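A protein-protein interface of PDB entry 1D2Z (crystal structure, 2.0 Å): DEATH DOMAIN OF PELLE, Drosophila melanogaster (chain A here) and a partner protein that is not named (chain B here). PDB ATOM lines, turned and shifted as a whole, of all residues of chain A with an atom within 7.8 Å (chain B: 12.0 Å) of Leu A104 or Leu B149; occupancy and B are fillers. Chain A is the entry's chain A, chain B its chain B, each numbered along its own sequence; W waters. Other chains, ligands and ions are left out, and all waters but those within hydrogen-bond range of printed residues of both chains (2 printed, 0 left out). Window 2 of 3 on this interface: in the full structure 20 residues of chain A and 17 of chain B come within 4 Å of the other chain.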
ATOM      1  N   LEU A   7      19.758   6.132   0.266  1.00  0.00           N
ATOM      2  CA  LEU A   7      18.350   5.775   0.610  1.00  0.00           C
ATOM      3  C   LEU A   7      17.406   6.039  -0.568  1.00  0.00           C
ATOM      4  O   LEU A   7      16.692   5.134  -1.011  1.00  0.00           O
ATOM      5  CB  LEU A   7      17.895   6.541   1.868  1.00  0.00           C
ATOM      6  CG  LEU A   7      16.549   6.199   2.531  1.00  0.00           C
ATOM      7  CD1 LEU A   7      16.619   6.460   4.034  1.00  0.00           C
ATOM      8  CD2 LEU A   7      15.412   6.993   1.901  1.00  0.00           C
ATOM      9  N   ASP A   8      17.409   7.269  -1.081  1.00  0.00           N
ATOM     10  CA  ASP A   8      16.546   7.620  -2.209  1.00  0.00           C
ATOM     11  C   ASP A   8      17.294   7.570  -3.539  1.00  0.00           C
ATOM     12  O   ASP A   8      17.899   8.553  -3.969  1.00  0.00           O
ATOM     13  CB  ASP A   8      15.906   9.004  -2.006  1.00  0.00           C
ATOM     14  CG  ASP A   8      14.736   9.271  -2.965  1.00  0.00           C
ATOM     15  OD1 ASP A   8      14.579   8.553  -3.979  1.00  0.00           O
ATOM     16  OD2 ASP A   8      13.957  10.209  -2.698  1.00  0.00           O
ATOM     17  N   THR A  10      15.646   6.545  -6.353  1.00  0.00           N
ATOM     18  CA  THR A  10      14.591   6.440  -7.356  1.00  0.00           C
ATOM     19  C   THR A  10      14.726   7.533  -8.401  1.00  0.00           C
ATOM     20  O   THR A  10      15.342   8.571  -8.152  1.00  0.00           O
ATOM     21  CB  THR A  10      13.186   6.511  -6.727  1.00  0.00           C
ATOM     22  OG1 THR A  10      13.009   7.767  -6.062  1.00  0.00           O
ATOM     23  CG2 THR A  10      12.991   5.375  -5.735  1.00  0.00           C
ATOM     24  N   VAL A  77      10.290   9.514  -7.538  1.00  0.00           N
ATOM     25  CA  VAL A  77       9.169   8.594  -7.442  1.00  0.00           C
ATOM     26  C   VAL A  77       8.984   8.178  -5.982  1.00  0.00           C
ATOM     27  O   VAL A  77       7.858   7.982  -5.530  1.00  0.00           O
ATOM     28  CB  VAL A  77       9.373   7.341  -8.337  1.00  0.00           C
ATOM     29  CG1 VAL A  77       8.197   6.404  -8.203  1.00  0.00           C
ATOM     30  CG2 VAL A  77       9.513   7.755  -9.789  1.00  0.00           C
ATOM     31  N   GLN A  78      10.081   8.071  -5.236  1.00  0.00           N
ATOM     32  CA  GLN A  78       9.973   7.695  -3.828  1.00  0.00           C
ATOM     33  C   GLN A  78       9.192   8.758  -3.052  1.00  0.00           C
ATOM     34  O   GLN A  78       8.332   8.433  -2.231  1.00  0.00           O
ATOM     35  CB  GLN A  78      11.352   7.481  -3.198  1.00  0.00           C
ATOM     36  CG  GLN A  78      11.273   6.996  -1.756  1.00  0.00           C
ATOM     37  CD  GLN A  78      12.629   6.755  -1.131  1.00  0.00           C
ATOM     38  OE1 GLN A  78      12.979   7.375  -0.130  1.00  0.00           O
ATOM     39  NE2 GLN A  78      13.395   5.838  -1.709  1.00  0.00           N
ATOM     40  N   THR A  79       9.465  10.028  -3.337  1.00  0.00           N
ATOM     41  CA  THR A  79       8.766  11.118  -2.662  1.00  0.00           C
ATOM     42  C   THR A  79       7.282  11.089  -3.035  1.00  0.00           C
ATOM     43  O   THR A  79       6.423  11.338  -2.194  1.00  0.00           O
ATOM     44  CB  THR A  79       9.418  12.484  -2.982  1.00  0.00           C
ATOM     45  OG1 THR A  79      10.779  12.455  -2.534  1.00  0.00           O
ATOM     46  CG2 THR A  79       8.696  13.625  -2.262  1.00  0.00           C
ATOM     47  N   PHE A  81       5.684   8.353  -3.809  1.00  0.00           N
ATOM     48  CA  PHE A  81       5.214   7.176  -3.077  1.00  0.00           C
ATOM     49  C   PHE A  81       4.826   7.604  -1.649  1.00  0.00           C
ATOM     50  O   PHE A  81       3.743   7.269  -1.162  1.00  0.00           O
ATOM     51  CB  PHE A  81       6.334   6.128  -3.053  1.00  0.00           C
ATOM     52  CG  PHE A  81       5.921   4.785  -2.506  1.00  0.00           C
ATOM     53  CD1 PHE A  81       5.245   3.865  -3.309  1.00  0.00           C
ATOM     54  CD2 PHE A  81       6.249   4.421  -1.201  1.00  0.00           C
ATOM     55  CE1 PHE A  81       4.904   2.598  -2.818  1.00  0.00           C
ATOM     56  CE2 PHE A  81       5.914   3.155  -0.700  1.00  0.00           C
ATOM     57  CZ  PHE A  81       5.240   2.244  -1.513  1.00  0.00           C
ATOM     58  N   ALA A  82       5.692   8.396  -1.011  1.00  0.00           N
ATOM     59  CA  ALA A  82       5.450   8.891   0.345  1.00  0.00           C
ATOM     60  C   ALA A  82       4.212   9.785   0.425  1.00  0.00           C
ATOM     61  O   ALA A  82       3.474   9.748   1.417  1.00  0.00           O
ATOM     62  CB  ALA A  82       6.679   9.642   0.866  1.00  0.00           C
ATOM     63  N   LEU A  83       3.984  10.592  -0.612  1.00  0.00           N
ATOM     64  CA  LEU A  83       2.817  11.468  -0.651  1.00  0.00           C
ATOM     65  C   LEU A  83       1.556  10.617  -0.701  1.00  0.00           C
ATOM     66  O   LEU A  83       0.584  10.888   0.006  1.00  0.00           O
ATOM     67  CB  LEU A  83       2.862  12.396  -1.866  1.00  0.00           C
ATOM     68  CG  LEU A  83       1.614  13.252  -2.137  1.00  0.00           C
ATOM     69  CD1 LEU A  83       1.325  14.195  -0.967  1.00  0.00           C
ATOM     70  CD2 LEU A  83       1.797  14.046  -3.426  1.00  0.00           C
ATOM     71  N   LYS A  85       1.282   7.627   0.310  1.00  0.00           N
ATOM     72  CA  LYS A  85       1.210   6.965   1.611  1.00  0.00           C
ATOM     73  C   LYS A  85       0.546   7.866   2.650  1.00  0.00           C
ATOM     74  O   LYS A  85      -0.314   7.413   3.410  1.00  0.00           O
ATOM     75  CB  LYS A  85       2.607   6.554   2.084  1.00  0.00           C
ATOM     76  CG  LYS A  85       2.620   5.788   3.404  1.00  0.00           C
ATOM     77  CD  LYS A  85       4.038   5.432   3.825  1.00  0.00           C
ATOM     78  CE  LYS A  85       4.063   4.659   5.149  1.00  0.00           C
ATOM     79  NZ  LYS A  85       3.611   5.467   6.321  1.00  0.00           N
ATOM     80  N   LYS A  86       0.918   9.146   2.647  1.00  0.00           N
ATOM     81  CA  LYS A  86       0.357  10.112   3.587  1.00  0.00           C
ATOM     82  C   LYS A  86      -1.133  10.335   3.344  1.00  0.00           C
ATOM     83  O   LYS A  86      -1.901  10.518   4.288  1.00  0.00           O
ATOM     84  CB  LYS A  86       1.119  11.447   3.515  1.00  0.00           C
ATOM     85  CG  LYS A  86       0.584  12.514   4.471  1.00  0.00           C
ATOM     86  CD  LYS A  86       1.620  13.583   4.817  1.00  0.00           C
ATOM     87  CE  LYS A  86       1.865  14.557   3.678  1.00  0.00           C
ATOM     88  NZ  LYS A  86       2.774  15.652   4.136  1.00  0.00           N
ATOM     89  N   MET A  93       0.030   3.828  -4.789  1.00  0.00           N
ATOM     90  CA  MET A  93       1.338   3.324  -4.366  1.00  0.00           C
ATOM     91  C   MET A  93       1.669   2.019  -5.101  1.00  0.00           C
ATOM     92  O   MET A  93       2.797   1.814  -5.549  1.00  0.00           O
ATOM     93  CB  MET A  93       1.339   3.051  -2.859  1.00  0.00           C
ATOM     94  CG  MET A  93       1.199   4.287  -1.991  1.00  0.00           C
ATOM     95  SD  MET A  93       0.728   3.896  -0.300  1.00  0.00           S
ATOM     96  CE  MET A  93       2.233   3.252   0.323  1.00  0.00           C
ATOM     97  N   LYS A  97       4.952   0.764  -7.489  1.00  0.00           N
ATOM     98  CA  LYS A  97       5.813  -0.067  -6.645  1.00  0.00           C
ATOM     99  C   LYS A  97       7.081  -0.543  -7.340  1.00  0.00           C
ATOM    100  O   LYS A  97       8.119  -0.692  -6.705  1.00  0.00           O
ATOM    101  CB  LYS A  97       5.048  -1.281  -6.103  1.00  0.00           C
ATOM    102  CG  LYS A  97       4.736  -2.349  -7.143  1.00  0.00           C
ATOM    103  CD  LYS A  97       3.845  -3.452  -6.571  1.00  0.00           C
ATOM    104  CE  LYS A  97       3.366  -4.405  -7.662  1.00  0.00           C
ATOM    105  NZ  LYS A  97       4.506  -5.107  -8.341  1.00  0.00           N
ATOM    106  N   TYR A  99       8.997   1.053  -9.324  1.00  0.00           N
ATOM    107  CA  TYR A  99       9.982   2.124  -9.498  1.00  0.00           C
ATOM    108  C   TYR A  99      10.472   2.644  -8.155  1.00  0.00           C
ATOM    109  O   TYR A  99      11.087   3.708  -8.062  1.00  0.00           O
ATOM    110  CB  TYR A  99       9.375   3.254 -10.319  1.00  0.00           C
ATOM    111  CG  TYR A  99       9.006   2.821 -11.713  1.00  0.00           C
ATOM    112  CD1 TYR A  99       9.945   2.858 -12.742  1.00  0.00           C
ATOM    113  CD2 TYR A  99       7.732   2.333 -11.996  1.00  0.00           C
ATOM    114  CE1 TYR A  99       9.628   2.413 -14.022  1.00  0.00           C
ATOM    115  CE2 TYR A  99       7.403   1.886 -13.270  1.00  0.00           C
ATOM    116  CZ  TYR A  99       8.357   1.928 -14.279  1.00  0.00           C
ATOM    117  OH  TYR A  99       8.045   1.478 -15.537  1.00  0.00           O
ATOM    118  N   VAL A 100      10.184   1.870  -7.118  1.00  0.00           N
ATOM    119  CA  VAL A 100      10.560   2.185  -5.748  1.00  0.00           C
ATOM    120  C   VAL A 100      11.183   0.913  -5.170  1.00  0.00           C
ATOM    121  O   VAL A 100      10.948  -0.184  -5.686  1.00  0.00           O
ATOM    122  CB  VAL A 100       9.301   2.585  -4.931  1.00  0.00           C
ATOM    123  CG1 VAL A 100       9.608   2.652  -3.468  1.00  0.00           C
ATOM    124  CG2 VAL A 100       8.767   3.933  -5.411  1.00  0.00           C
ATOM    125  N   SER A 101      12.000   1.064  -4.129  1.00  0.00           N
ATOM    126  CA  SER A 101      12.654  -0.076  -3.485  1.00  0.00           C
ATOM    127  C   SER A 101      11.645  -1.058  -2.903  1.00  0.00           C
ATOM    128  O   SER A 101      10.643  -0.656  -2.307  1.00  0.00           O
ATOM    129  CB  SER A 101      13.598   0.403  -2.379  1.00  0.00           C
ATOM    130  OG  SER A 101      14.111  -0.695  -1.648  1.00  0.00           O
ATOM    131  N   GLU A 102      11.935  -2.346  -3.070  1.00  0.00           N
ATOM    132  CA  GLU A 102      11.076  -3.423  -2.576  1.00  0.00           C
ATOM    133  C   GLU A 102      10.845  -3.345  -1.071  1.00  0.00           C
ATOM    134  O   GLU A 102       9.806  -3.777  -0.577  1.00  0.00           O
ATOM    135  CB  GLU A 102      11.677  -4.788  -2.923  1.00  0.00           C
ATOM    136  CG  GLU A 102      11.823  -5.053  -4.411  1.00  0.00           C
ATOM    137  CD  GLU A 102      12.408  -6.428  -4.718  1.00  0.00           C
ATOM    138  OE1 GLU A 102      12.973  -7.070  -3.803  1.00  0.00           O
ATOM    139  OE2 GLU A 102      12.307  -6.862  -5.887  1.00  0.00           O
ATOM    140  N   ASP A 103      11.822  -2.795  -0.353  1.00  0.00           N
ATOM    141  CA  ASP A 103      11.746  -2.651   1.100  1.00  0.00           C
ATOM    142  C   ASP A 103      10.616  -1.728   1.544  1.00  0.00           C
ATOM    143  O   ASP A 103      10.279  -1.681   2.731  1.00  0.00           O
ATOM    144  CB  ASP A 103      13.075  -2.125   1.653  1.00  0.00           C
ATOM    145  CG  ASP A 103      14.257  -3.007   1.282  1.00  0.00           C
ATOM    146  OD1 ASP A 103      14.092  -4.247   1.219  1.00  0.00           O
ATOM    147  OD2 ASP A 103      15.357  -2.459   1.058  1.00  0.00           O
ATOM    148  N   LEU A 104      10.036  -0.993   0.596  1.00  0.00           N
ATOM    149  CA  LEU A 104       8.940  -0.073   0.901  1.00  0.00           C
ATOM    150  C   LEU A 104       7.566  -0.665   0.584  1.00  0.00           C
ATOM    151  O   LEU A 104       6.537  -0.078   0.919  1.00  0.00           O
ATOM    152  CB  LEU A 104       9.132   1.249   0.152  1.00  0.00           C
ATOM    153  CG  LEU A 104      10.439   1.995   0.452  1.00  0.00           C
ATOM    154  CD1 LEU A 104      10.517   3.257  -0.382  1.00  0.00           C
ATOM    155  CD2 LEU A 104      10.531   2.332   1.934  1.00  0.00           C
ATOM    156  N   HIS A 105       7.557  -1.848  -0.024  1.00  0.00           N
ATOM    157  CA  HIS A 105       6.313  -2.515  -0.394  1.00  0.00           C
ATOM    158  C   HIS A 105       5.445  -2.936   0.792  1.00  0.00           C
ATOM    159  O   HIS A 105       4.277  -3.292   0.617  1.00  0.00           O
ATOM    160  CB  HIS A 105       6.604  -3.708  -1.310  1.00  0.00           C
ATOM    161  CG  HIS A 105       7.185  -3.318  -2.635  1.00  0.00           C
ATOM    162  ND1 HIS A 105       7.476  -4.238  -3.620  1.00  0.00           N
ATOM    163  CD2 HIS A 105       7.530  -2.109  -3.137  1.00  0.00           C
ATOM    164  CE1 HIS A 105       7.975  -3.611  -4.671  1.00  0.00           C
ATOM    165  NE2 HIS A 105       8.019  -2.318  -4.404  1.00  0.00           N
ATOM    166  N   LYS A 106       6.012  -2.870   1.996  1.00  0.00           N
ATOM    167  CA  LYS A 106       5.298  -3.224   3.223  1.00  0.00           C
ATOM    168  C   LYS A 106       4.166  -2.243   3.518  1.00  0.00           C
ATOM    169  O   LYS A 106       3.127  -2.620   4.062  1.00  0.00           O
ATOM    170  CB  LYS A 106       6.263  -3.226   4.415  1.00  0.00           C
ATOM    171  CG  LYS A 106       7.308  -4.318   4.367  1.00  0.00           C
ATOM    172  CD  LYS A 106       8.344  -4.165   5.472  1.00  0.00           C
ATOM    173  CE  LYS A 106       9.390  -5.273   5.393  1.00  0.00           C
ATOM    174  NZ  LYS A 106      10.430  -5.158   6.456  1.00  0.00           N
ATOM    175  N   TYR A 107       4.375  -0.984   3.142  1.00  0.00           N
ATOM    176  CA  TYR A 107       3.400   0.076   3.380  1.00  0.00           C
ATOM    177  C   TYR A 107       2.208   0.067   2.426  1.00  0.00           C
ATOM    178  O   TYR A 107       1.219   0.765   2.658  1.00  0.00           O
ATOM    179  CB  TYR A 107       4.090   1.438   3.317  1.00  0.00           C
ATOM    180  CG  TYR A 107       5.374   1.518   4.111  1.00  0.00           C
ATOM    181  CD1 TYR A 107       5.404   1.195   5.470  1.00  0.00           C
ATOM    182  CD2 TYR A 107       6.562   1.922   3.502  1.00  0.00           C
ATOM    183  CE1 TYR A 107       6.592   1.276   6.203  1.00  0.00           C
ATOM    184  CE2 TYR A 107       7.750   2.006   4.222  1.00  0.00           C
ATOM    185  CZ  TYR A 107       7.760   1.684   5.570  1.00  0.00           C
ATOM    186  OH  TYR A 107       8.938   1.781   6.278  1.00  0.00           O
ATOM    187  N   ILE A 108       2.306  -0.711   1.352  1.00  0.00           N
ATOM    188  CA  ILE A 108       1.231  -0.793   0.368  1.00  0.00           C
ATOM    189  C   ILE A 108       0.046  -1.611   0.892  1.00  0.00           C
ATOM    190  O   ILE A 108      -1.099  -1.118   0.790  1.00  0.00           O
ATOM    191  CB  ILE A 108       1.737  -1.401  -0.955  1.00  0.00           C
ATOM    192  CG1 ILE A 108       2.923  -0.590  -1.480  1.00  0.00           C
ATOM    193  CG2 ILE A 108       0.618  -1.428  -1.990  1.00  0.00           C
ATOM    194  CD1 ILE A 108       3.598  -1.199  -2.679  1.00  0.00           C
ATOM    195  OXT ILE A 108       0.276  -2.732   1.398  1.00  0.00           O
ATOM    196  N   VAL B 140      11.708  22.813   4.654  1.00  0.00           N
ATOM    197  CA  VAL B 140      11.000  21.791   5.428  1.00  0.00           C
ATOM    198  C   VAL B 140       9.528  21.731   5.047  1.00  0.00           C
ATOM    199  O   VAL B 140       8.908  20.672   5.103  1.00  0.00           O
ATOM    200  CB  VAL B 140      11.113  22.014   6.970  1.00  0.00           C
ATOM    201  CG1 VAL B 140      12.545  21.803   7.429  1.00  0.00           C
ATOM    202  CG2 VAL B 140      10.621  23.399   7.359  1.00  0.00           C
ATOM    203  N   ALA B 145       9.622  20.750  -0.517  1.00  0.00           N
ATOM    204  CA  ALA B 145      10.064  19.877   0.566  1.00  0.00           C
ATOM    205  C   ALA B 145       9.865  18.392   0.295  1.00  0.00           C
ATOM    206  O   ALA B 145       8.939  17.986  -0.413  1.00  0.00           O
ATOM    207  CB  ALA B 145       9.357  20.255   1.859  1.00  0.00           C
ATOM    208  N   LEU B 146      10.730  17.592   0.904  1.00  0.00           N
ATOM    209  CA  LEU B 146      10.673  16.143   0.788  1.00  0.00           C
ATOM    210  C   LEU B 146       9.605  15.646   1.759  1.00  0.00           C
ATOM    211  O   LEU B 146       9.168  16.383   2.652  1.00  0.00           O
ATOM    212  CB  LEU B 146      12.031  15.537   1.147  1.00  0.00           C
ATOM    213  CG  LEU B 146      13.239  16.146   0.429  1.00  0.00           C
ATOM    214  CD1 LEU B 146      14.522  15.473   0.899  1.00  0.00           C
ATOM    215  CD2 LEU B 146      13.076  16.014  -1.081  1.00  0.00           C
ATOM    216  N   ILE B 147       9.158  14.412   1.560  1.00  0.00           N
ATOM    217  CA  ILE B 147       8.141  13.815   2.418  1.00  0.00           C
ATOM    218  C   ILE B 147       8.695  12.506   2.978  1.00  0.00           C
ATOM    219  O   ILE B 147       9.188  11.660   2.231  1.00  0.00           O
ATOM    220  CB  ILE B 147       6.834  13.543   1.632  1.00  0.00           C
ATOM    221  CG1 ILE B 147       6.358  14.832   0.952  1.00  0.00           C
ATOM    222  CG2 ILE B 147       5.750  13.019   2.569  1.00  0.00           C
ATOM    223  CD1 ILE B 147       5.125  14.670   0.096  1.00  0.00           C
ATOM    224  N   SER B 148       8.649  12.362   4.297  1.00  0.00           N
ATOM    225  CA  SER B 148       9.158  11.160   4.950  1.00  0.00           C
ATOM    226  C   SER B 148       8.115  10.049   5.013  1.00  0.00           C
ATOM    227  O   SER B 148       6.912  10.312   5.016  1.00  0.00           O
ATOM    228  CB  SER B 148       9.634  11.486   6.368  1.00  0.00           C
ATOM    229  OG  SER B 148       8.544  11.882   7.183  1.00  0.00           O
ATOM    230  N   LEU B 149       8.592   8.810   5.065  1.00  0.00           N
ATOM    231  CA  LEU B 149       7.715   7.649   5.152  1.00  0.00           C
ATOM    232  C   LEU B 149       7.708   7.147   6.595  1.00  0.00           C
ATOM    233  O   LEU B 149       8.753   6.768   7.131  1.00  0.00           O
ATOM    234  CB  LEU B 149       8.195   6.530   4.218  1.00  0.00           C
ATOM    235  CG  LEU B 149       8.388   6.823   2.726  1.00  0.00           C
ATOM    236  CD1 LEU B 149       9.746   7.469   2.491  1.00  0.00           C
ATOM    237  CD2 LEU B 149       8.294   5.530   1.936  1.00  0.00           C
ATOM    238  N   GLU B 150       6.540   7.176   7.229  1.00  0.00           N
ATOM    239  CA  GLU B 150       6.402   6.719   8.613  1.00  0.00           C
ATOM    240  C   GLU B 150       6.508   5.199   8.725  1.00  0.00           C
ATOM    241  O   GLU B 150       7.214   4.740   9.650  1.00  0.00           O
ATOM    242  CB  GLU B 150       5.069   7.193   9.206  1.00  0.00           C
ATOM    243  CG  GLU B 150       5.053   8.648   9.660  1.00  0.00           C
ATOM    244  CD  GLU B 150       5.370   9.625   8.545  1.00  0.00           C
ATOM    245  OE1 GLU B 150       4.558   9.740   7.602  1.00  0.00           O
ATOM    246  OE2 GLU B 150       6.432  10.279   8.616  1.00  0.00           O
HETATM  247  O   HOH W   1      10.675  12.440   0.258  1.00  0.00           O
HETATM  248  O   HOH W   2       4.314   9.059   4.073  1.00  0.00           O
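OG of Ser B148 lies within hydrogen-bond range of OE2 of Glu B150 (3.0 Å).
Among the printed residues, pairs that only touch across the chains: Ala A82 with Ile B147 (3.5 Å), Lys A85 with Glu B150 (3.5 Å), Leu A83 with Ile B147 (3.8 Å), Ala A82 with Leu B149 (3.8 Å), Leu A104 with Leu B149 (3.9 Å), Phe A81 with Leu B149 (3.9 Å) and Thr A79 with Ile B147 (3.9 Å).
Leu A104 touches just one residue of chain B: Leu B149 (3.9 Å).
Of chain A, only Phe A81 (3.9 Å), Ala A82 (3.8 Å) and Leu A104 (3.9 Å) come within 4 Å of Leu B149.
Thr A79 touches one residue of chain B.
Printed residues of chain B within 4 Å of Phe A81: Leu B149.
Of chain B, only Ile B147 and Leu B149 come within 4 Å of Ala A82.
No residue of chain B comes within 4 Å of Ser A101.
No residue of chain B comes within 4 Å of Asp A103.
His A105 touches none of the printed residues of chain B.
No residue of chain B comes within 4 Å of Lys A106.
No residue of chain B comes within 4 Å of Ile A108.
Of the printed residues of chain B, Lys A85 touches Glu B150.
Of the printed residues of chain A, Ile B147 touches Thr A79 (3.9 Å), Ala A82 (3.5 Å) and Leu A83 (3.8 Å).
Of the printed residues of chain A, Glu B150 touches Lys A85.
Lys A97 touches none of the printed residues of chain B.
The nearest printed residue of chain A that does not touch Ile B147 is Lys A86 (4.3 Å).
Printed residues of chain A that touch a printed residue of chain B: Thr A79, Phe A81, Ala A82, Leu A83, Lys A85 and Leu A104.
Hydrophobic or aromatic side chains of chain A within 4 Å of the printed part of chain B: Phe A81, Ala A82, Leu A83 and Leu A104.
Among the printed residues, 7 pairs touch across the chains.
Among the printed residues, no Asp or Glu carboxylate lies within 4 Å of a Lys or Arg side-chain nitrogen of the other chain.
Water W1 lies within hydrogen-bond range of O of Ile B147 (2.6 Å) and OG1 of Thr A79 (2.8 Å).
Water W2 lies within hydrogen-bond range of the backbone carbonyl oxygen of Ala A82 and the backbone carbonyl oxygen of Ser B148.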
